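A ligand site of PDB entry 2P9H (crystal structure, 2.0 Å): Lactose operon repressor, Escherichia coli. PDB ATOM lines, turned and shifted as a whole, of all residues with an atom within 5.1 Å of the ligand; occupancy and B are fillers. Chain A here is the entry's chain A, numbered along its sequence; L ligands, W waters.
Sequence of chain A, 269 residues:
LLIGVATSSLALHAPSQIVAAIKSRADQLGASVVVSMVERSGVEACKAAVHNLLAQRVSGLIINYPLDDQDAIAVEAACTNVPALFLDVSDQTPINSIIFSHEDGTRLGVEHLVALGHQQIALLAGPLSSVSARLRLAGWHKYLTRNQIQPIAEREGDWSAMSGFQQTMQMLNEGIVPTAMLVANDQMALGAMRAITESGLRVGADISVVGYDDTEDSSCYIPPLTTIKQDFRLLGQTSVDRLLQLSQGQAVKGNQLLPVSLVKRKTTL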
ATOM      1  N   SER A   8      18.058   8.318  28.317  1.00  0.00           N
ATOM      2  CA  SER A   8      19.270   7.664  28.765  1.00  0.00           C
ATOM      3  C   SER A   8      19.399   7.840  30.282  1.00  0.00           C
ATOM      4  O   SER A   8      18.678   8.611  30.884  1.00  0.00           O
ATOM      5  CB  SER A   8      20.447   8.254  28.016  1.00  0.00           C
ATOM      6  OG  SER A   8      20.297   9.630  27.946  1.00  0.00           O
ATOM      7  N   LEU A  12      23.089  10.185  35.005  1.00  0.00           N
ATOM      8  CA  LEU A  12      23.823  11.258  34.369  1.00  0.00           C
ATOM      9  C   LEU A  12      23.004  12.492  34.542  1.00  0.00           C
ATOM     10  O   LEU A  12      21.769  12.468  34.425  1.00  0.00           O
ATOM     11  CB  LEU A  12      24.103  10.924  32.894  1.00  0.00           C
ATOM     12  CG  LEU A  12      25.096   9.772  32.682  1.00  0.00           C
ATOM     13  CD1 LEU A  12      25.254   9.525  31.190  1.00  0.00           C
ATOM     14  CD2 LEU A  12      26.456  10.080  33.378  1.00  0.00           C
ATOM     15  N   HIS A  13      23.662  13.568  34.881  1.00  0.00           N
ATOM     16  CA  HIS A  13      22.963  14.758  35.289  1.00  0.00           C
ATOM     17  C   HIS A  13      22.243  15.506  34.148  1.00  0.00           C
ATOM     18  O   HIS A  13      21.224  16.136  34.413  1.00  0.00           O
ATOM     19  CB  HIS A  13      23.918  15.727  35.998  1.00  0.00           C
ATOM     20  CG  HIS A  13      24.699  15.104  37.116  1.00  0.00           C
ATOM     21  ND1 HIS A  13      24.269  13.961  37.774  1.00  0.00           N
ATOM     22  CD2 HIS A  13      25.849  15.482  37.718  1.00  0.00           C
ATOM     23  CE1 HIS A  13      25.141  13.656  38.725  1.00  0.00           C
ATOM     24  NE2 HIS A  13      26.119  14.561  38.710  1.00  0.00           N
ATOM     25  N   ALA A  14      22.747  15.424  32.917  1.00  0.00           N
ATOM     26  CA  ALA A  14      22.083  16.206  31.849  1.00  0.00           C
ATOM     27  C   ALA A  14      20.687  15.601  31.576  1.00  0.00           C
ATOM     28  O   ALA A  14      19.721  16.344  31.517  1.00  0.00           O
ATOM     29  CB  ALA A  14      22.906  16.261  30.560  1.00  0.00           C
ATOM     30  N   PRO A  15      20.581  14.260  31.404  1.00  0.00           N
ATOM     31  CA  PRO A  15      19.252  13.658  31.149  1.00  0.00           C
ATOM     32  C   PRO A  15      18.256  13.961  32.269  1.00  0.00           C
ATOM     33  O   PRO A  15      17.057  14.120  31.979  1.00  0.00           O
ATOM     34  CB  PRO A  15      19.523  12.159  31.134  1.00  0.00           C
ATOM     35  CG  PRO A  15      20.975  12.011  30.810  1.00  0.00           C
ATOM     36  CD  PRO A  15      21.668  13.278  31.287  1.00  0.00           C
ATOM     37  N   ILE A  18      17.094  17.495  31.802  1.00  0.00           N
ATOM     38  CA  ILE A  18      16.199  17.552  30.648  1.00  0.00           C
ATOM     39  C   ILE A  18      14.797  17.039  31.013  1.00  0.00           C
ATOM     40  O   ILE A  18      13.789  17.650  30.708  1.00  0.00           O
ATOM     41  CB  ILE A  18      16.822  16.755  29.486  1.00  0.00           C
ATOM     42  CG1 ILE A  18      18.161  17.403  29.101  1.00  0.00           C
ATOM     43  CG2 ILE A  18      15.810  16.637  28.306  1.00  0.00           C
ATOM     44  CD1 ILE A  18      18.848  16.750  27.905  1.00  0.00           C
ATOM     45  N   ASN A  64      15.051  11.045  24.440  1.00  0.00           N
ATOM     46  CA  ASN A  64      16.375  11.612  24.825  1.00  0.00           C
ATOM     47  C   ASN A  64      17.347  10.498  25.095  1.00  0.00           C
ATOM     48  O   ASN A  64      17.533  10.057  26.232  1.00  0.00           O
ATOM     49  CB  ASN A  64      16.307  12.552  26.009  1.00  0.00           C
ATOM     50  CG  ASN A  64      17.691  13.064  26.400  1.00  0.00           C
ATOM     51  OD1 ASN A  64      18.587  13.156  25.565  1.00  0.00           O
ATOM     52  ND2 ASN A  64      17.883  13.321  27.676  1.00  0.00           N
ATOM     53  N   PRO A  66      20.813   8.501  22.854  1.00  0.00           N
ATOM     54  CA  PRO A  66      21.658   8.640  21.665  1.00  0.00           C
ATOM     55  C   PRO A  66      21.344   7.556  20.650  1.00  0.00           C
ATOM     56  O   PRO A  66      21.443   6.354  20.931  1.00  0.00           O
ATOM     57  CB  PRO A  66      23.087   8.456  22.227  1.00  0.00           C
ATOM     58  CG  PRO A  66      22.877   7.566  23.455  1.00  0.00           C
ATOM     59  CD  PRO A  66      21.584   8.025  24.022  1.00  0.00           C
ATOM     60  N   LEU A  87      16.041  13.833  20.725  1.00  0.00           N
ATOM     61  CA  LEU A  87      16.840  14.899  21.335  1.00  0.00           C
ATOM     62  C   LEU A  87      18.320  14.638  21.322  1.00  0.00           C
ATOM     63  O   LEU A  87      19.094  15.552  21.598  1.00  0.00           O
ATOM     64  CB  LEU A  87      16.374  15.184  22.766  1.00  0.00           C
ATOM     65  CG  LEU A  87      14.963  15.712  23.015  1.00  0.00           C
ATOM     66  CD1 LEU A  87      14.929  16.223  24.480  1.00  0.00           C
ATOM     67  CD2 LEU A  87      14.496  16.848  22.025  1.00  0.00           C
ATOM     68  N   ASP A  88      18.695  13.410  21.029  1.00  0.00           N
ATOM     69  CA  ASP A  88      20.083  12.984  21.043  1.00  0.00           C
ATOM     70  C   ASP A  88      20.411  12.244  19.736  1.00  0.00           C
ATOM     71  O   ASP A  88      20.636  11.024  19.704  1.00  0.00           O
ATOM     72  CB  ASP A  88      20.364  12.073  22.242  1.00  0.00           C
ATOM     73  CG  ASP A  88      21.848  11.879  22.464  1.00  0.00           C
ATOM     74  OD1 ASP A  88      22.654  12.086  21.466  1.00  0.00           O
ATOM     75  OD2 ASP A  88      22.200  11.500  23.609  1.00  0.00           O
ATOM     76  N   SER A 132      26.050  11.911  19.904  1.00  0.00           N
ATOM     77  CA  SER A 132      26.350  13.261  20.356  1.00  0.00           C
ATOM     78  C   SER A 132      27.817  13.386  20.790  1.00  0.00           C
ATOM     79  O   SER A 132      28.411  14.436  20.593  1.00  0.00           O
ATOM     80  CB  SER A 132      25.401  13.718  21.493  1.00  0.00           C
ATOM     81  OG  SER A 132      24.126  14.137  20.999  1.00  0.00           O
ATOM     82  N   ARG A 136      30.649  15.890  18.909  1.00  0.00           N
ATOM     83  CA  ARG A 136      31.381  16.922  19.657  1.00  0.00           C
ATOM     84  C   ARG A 136      32.843  16.700  19.388  1.00  0.00           C
ATOM     85  O   ARG A 136      33.572  17.643  19.202  1.00  0.00           O
ATOM     86  CB  ARG A 136      31.088  16.829  21.174  1.00  0.00           C
ATOM     87  CG  ARG A 136      29.722  17.395  21.540  1.00  0.00           C
ATOM     88  CD  ARG A 136      29.385  17.133  22.982  1.00  0.00           C
ATOM     89  NE  ARG A 136      27.954  17.189  23.173  1.00  0.00           N
ATOM     90  CZ  ARG A 136      27.328  16.854  24.295  1.00  0.00           C
ATOM     91  NH1 ARG A 136      28.021  16.395  25.357  1.00  0.00           N
ATOM     92  NH2 ARG A 136      26.001  16.936  24.349  1.00  0.00           N
ATOM     93  N   TRP A 159      30.964   9.448  30.284  1.00  0.00           N
ATOM     94  CA  TRP A 159      30.118  10.559  30.749  1.00  0.00           C
ATOM     95  C   TRP A 159      30.123  10.715  32.288  1.00  0.00           C
ATOM     96  O   TRP A 159      29.616  11.703  32.778  1.00  0.00           O
ATOM     97  CB  TRP A 159      28.649  10.357  30.335  1.00  0.00           C
ATOM     98  CG  TRP A 159      28.229  10.379  28.874  1.00  0.00           C
ATOM     99  CD1 TRP A 159      27.489   9.406  28.248  1.00  0.00           C
ATOM    100  CD2 TRP A 159      28.459  11.421  27.880  1.00  0.00           C
ATOM    101  NE1 TRP A 159      27.261   9.762  26.957  1.00  0.00           N
ATOM    102  CE2 TRP A 159      27.811  10.998  26.708  1.00  0.00           C
ATOM    103  CE3 TRP A 159      29.145  12.642  27.872  1.00  0.00           C
ATOM    104  CZ2 TRP A 159      27.829  11.750  25.489  1.00  0.00           C
ATOM    105  CZ3 TRP A 159      29.145  13.418  26.666  1.00  0.00           C
ATOM    106  CH2 TRP A 159      28.498  12.952  25.509  1.00  0.00           C
ATOM    107  N   ALA A 184      33.855  16.473  27.145  1.00  0.00           N
ATOM    108  CA  ALA A 184      32.562  16.365  26.464  1.00  0.00           C
ATOM    109  C   ALA A 184      31.357  16.497  27.368  1.00  0.00           C
ATOM    110  O   ALA A 184      30.256  16.709  26.851  1.00  0.00           O
ATOM    111  CB  ALA A 184      32.471  15.136  25.641  1.00  0.00           C
ATOM    112  N   ASN A 185      31.557  16.317  28.692  1.00  0.00           N
ATOM    113  CA  ASN A 185      30.572  16.799  29.665  1.00  0.00           C
ATOM    114  C   ASN A 185      31.134  17.373  30.970  1.00  0.00           C
ATOM    115  O   ASN A 185      32.337  17.314  31.200  1.00  0.00           O
ATOM    116  CB  ASN A 185      29.404  15.814  29.875  1.00  0.00           C
ATOM    117  CG  ASN A 185      29.747  14.697  30.808  1.00  0.00           C
ATOM    118  OD1 ASN A 185      30.917  14.483  31.140  1.00  0.00           O
ATOM    119  ND2 ASN A 185      28.745  13.974  31.268  1.00  0.00           N
ATOM    120  N   GLN A 187      30.284  16.334  34.031  1.00  0.00           N
ATOM    121  CA  GLN A 187      30.626  15.253  35.009  1.00  0.00           C
ATOM    122  C   GLN A 187      32.032  14.678  34.842  1.00  0.00           C
ATOM    123  O   GLN A 187      32.782  14.497  35.835  1.00  0.00           O
ATOM    124  CB  GLN A 187      29.598  14.118  35.026  1.00  0.00           C
ATOM    125  CG  GLN A 187      28.207  14.514  35.496  1.00  0.00           C
ATOM    126  CD  GLN A 187      27.258  13.320  35.496  1.00  0.00           C
ATOM    127  OE1 GLN A 187      26.373  13.216  34.657  1.00  0.00           O
ATOM    128  NE2 GLN A 187      27.497  12.364  36.419  1.00  0.00           N
ATOM    129  N   TYR A 212      31.129  20.637  29.310  1.00  0.00           N
ATOM    130  CA  TYR A 212      30.104  20.663  28.305  1.00  0.00           C
ATOM    131  C   TYR A 212      28.792  20.344  28.995  1.00  0.00           C
ATOM    132  O   TYR A 212      28.696  19.315  29.677  1.00  0.00           O
ATOM    133  CB  TYR A 212      30.424  19.672  27.192  1.00  0.00           C
ATOM    134  CG  TYR A 212      29.965  20.116  25.836  1.00  0.00           C
ATOM    135  CD1 TYR A 212      28.613  20.099  25.482  1.00  0.00           C
ATOM    136  CD2 TYR A 212      30.891  20.573  24.887  1.00  0.00           C
ATOM    137  CE1 TYR A 212      28.180  20.492  24.217  1.00  0.00           C
ATOM    138  CE2 TYR A 212      30.487  20.978  23.593  1.00  0.00           C
ATOM    139  CZ  TYR A 212      29.143  20.941  23.271  1.00  0.00           C
ATOM    140  OH  TYR A 212      28.721  21.381  22.025  1.00  0.00           O
ATOM    141  N   ASP A 213      27.821  21.259  28.866  1.00  0.00           N
ATOM    142  CA  ASP A 213      26.445  21.155  29.429  1.00  0.00           C
ATOM    143  C   ASP A 213      26.056  22.324  30.299  1.00  0.00           C
ATOM    144  O   ASP A 213      24.891  22.759  30.256  1.00  0.00           O
ATOM    145  CB  ASP A 213      26.238  19.913  30.278  1.00  0.00           C
ATOM    146  CG  ASP A 213      26.094  18.689  29.456  1.00  0.00           C
ATOM    147  OD1 ASP A 213      25.837  18.831  28.226  1.00  0.00           O
ATOM    148  OD2 ASP A 213      26.250  17.609  30.071  1.00  0.00           O
ATOM    149  N   GLN A 230      24.369  24.331  27.647  1.00  0.00           N
ATOM    150  CA  GLN A 230      23.274  23.887  26.808  1.00  0.00           C
ATOM    151  C   GLN A 230      22.082  24.101  27.697  1.00  0.00           C
ATOM    152  O   GLN A 230      21.981  23.491  28.783  1.00  0.00           O
ATOM    153  CB  GLN A 230      23.456  22.399  26.449  1.00  0.00           C
ATOM    154  CG  GLN A 230      24.706  22.123  25.627  1.00  0.00           C
ATOM    155  CD  GLN A 230      24.711  20.735  25.040  1.00  0.00           C
ATOM    156  OE1 GLN A 230      24.838  19.707  25.753  1.00  0.00           O
ATOM    157  NE2 GLN A 230      24.554  20.673  23.734  1.00  0.00           N
ATOM    158  N   PHE A 232      18.967  23.323  29.015  1.00  0.00           N
ATOM    159  CA  PHE A 232      18.008  22.215  29.104  1.00  0.00           C
ATOM    160  C   PHE A 232      16.576  22.704  29.391  1.00  0.00           C
ATOM    161  O   PHE A 232      15.596  22.105  28.936  1.00  0.00           O
ATOM    162  CB  PHE A 232      18.477  21.209  30.151  1.00  0.00           C
ATOM    163  CG  PHE A 232      19.867  20.714  29.894  1.00  0.00           C
ATOM    164  CD1 PHE A 232      20.196  20.154  28.651  1.00  0.00           C
ATOM    165  CD2 PHE A 232      20.866  20.876  30.843  1.00  0.00           C
ATOM    166  CE1 PHE A 232      21.492  19.724  28.397  1.00  0.00           C
ATOM    167  CE2 PHE A 232      22.154  20.493  30.569  1.00  0.00           C
ATOM    168  CZ  PHE A 232      22.480  19.895  29.362  1.00  0.00           C
ATOM    169  N   LEU A 235      15.511  23.432  26.031  1.00  0.00           N
ATOM    170  CA  LEU A 235      15.274  22.155  25.398  1.00  0.00           C
ATOM    171  C   LEU A 235      13.921  21.566  25.804  1.00  0.00           C
ATOM    172  O   LEU A 235      13.175  21.034  24.963  1.00  0.00           O
ATOM    173  CB  LEU A 235      16.381  21.156  25.730  1.00  0.00           C
ATOM    174  CG  LEU A 235      16.290  19.835  24.966  1.00  0.00           C
ATOM    175  CD1 LEU A 235      16.359  20.078  23.459  1.00  0.00           C
ATOM    176  CD2 LEU A 235      17.425  18.922  25.374  1.00  0.00           C
HETATM  177  C1  LIG L   1      24.155  14.587  26.791  1.00  0.00           C
HETATM  178  C2  LIG L   1      25.062  15.310  27.816  1.00  0.00           C
HETATM  179  O1  LIG L   1      25.732  16.404  27.122  1.00  0.00           O
HETATM  180  C3  LIG L   1      26.069  14.324  28.401  1.00  0.00           C
HETATM  181  O2  LIG L   1      26.752  14.883  29.538  1.00  0.00           O
HETATM  182  C4  LIG L   1      25.402  12.993  28.807  1.00  0.00           C
HETATM  183  O3  LIG L   1      24.611  13.283  29.954  1.00  0.00           O
HETATM  184  C5  LIG L   1      24.451  12.504  27.685  1.00  0.00           C
HETATM  185  O4  LIG L   1      23.483  13.581  27.414  1.00  0.00           O
HETATM  186  C6  LIG L   1      23.701  11.246  28.056  1.00  0.00           C
HETATM  187  O5  LIG L   1      23.362  10.573  26.805  1.00  0.00           O
HETATM  188  S1  LIG L   1      22.917  15.785  26.310  1.00  0.00           S
HETATM  189  C7  LIG L   1      21.989  14.929  24.983  1.00  0.00           C
HETATM  190  C8  LIG L   1      20.642  15.645  24.814  1.00  0.00           C
HETATM  191  C9  LIG L   1      22.786  14.956  23.667  1.00  0.00           C
HETATM  192  O   HOH W   1      24.735  11.089  24.357  1.00  0.00           O
HETATM  193  O   HOH W   2      20.438  11.344  25.791  1.00  0.00           O
HETATM  194  O   HOH W   3      20.575  13.829  27.910  1.00  0.00           O
HETATM  195  O   HOH W   4      25.681  14.773  32.598  1.00  0.00           O
HETATM  196  O   HOH W   5      23.412   7.836  27.104  1.00  0.00           O
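Residues that only touch the ligand: Ser 132 (3.1 Å), Pro 15 (3.2 Å), Asn 64 (3.3 Å), Asp 88 (3.4 Å), Ala 14 (3.5 Å), Trp 159 (3.5 Å), Leu 87 (3.6 Å), Gln 230 (3.7 Å), Ile 18 (3.7 Å) and Leu 12 (3.8 Å). 14 residues have an atom within 4 Å of the ligand: Ser 8, Leu 12, Ala 14, Pro 15, Ile 18, Asn 64, Leu 87, Asp 88, Ser 132, Arg 136, Trp 159, Asn 185, Asp 213 and Gln 230.
The side-chain carboxylate (OD1) of Asp 213 sits close to the side-chain amide oxygen (OE1) of Gln 230. The side-chain amide nitrogen (ND2) of Asn 185 is in hydrogen-bond range of the backbone carbonyl oxygen (O) of Trp 159. The side-chain amide oxygen (OD1) of Asn 185 sits close to the backbone NH (N) of Gln 187. OE1 of Gln 230 sits at hydrogen-bond distance from NH2 of Arg 136 (3.3 Å). The guanidinium group of Arg 136 is in hydrogen-bond range of the backbone carbonyl oxygen of Ala 184, 2.7 Å away. OG of Ser 132 lies within hydrogen-bond range of OD1 of Asp 88 (2.6 Å). The backbone NH (N) of Ser 8 is in hydrogen-bond range of the backbone carbonyl oxygen (O) of Asn 64 (2.8 Å).
Water W1 bridges OD2 of Asp 88 (2.7 Å) and O5 of the ligand (2.9 Å). Water W3 bridges the side-chain amide nitrogen (ND2) of Asn 64 and an oxygen (O4) of the ligand. Water W2 lies within hydrogen-bond range of OD1 of Asn 64 (2.6 Å), OG of Ser 8 (2.8 Å), OD2 of Asp 88 (2.8 Å) and O5 of the ligand (3.2 Å).
The side-chain carboxylate of Asp 213 is in hydrogen-bond range of an oxygen (O1) of the ligand (2.7 Å). The side-chain amide nitrogen (ND2) of Asn 185 lies within hydrogen-bond range of an oxygen (O2) of the ligand, 2.8 Å away. An oxygen (O1) of the ligand is in hydrogen-bond range of the guanidinium group (NH2) of Arg 136 (2.8 Å). An oxygen (O5) of the ligand lies within hydrogen-bond range of the side-chain hydroxyl (OG) of Ser 8.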
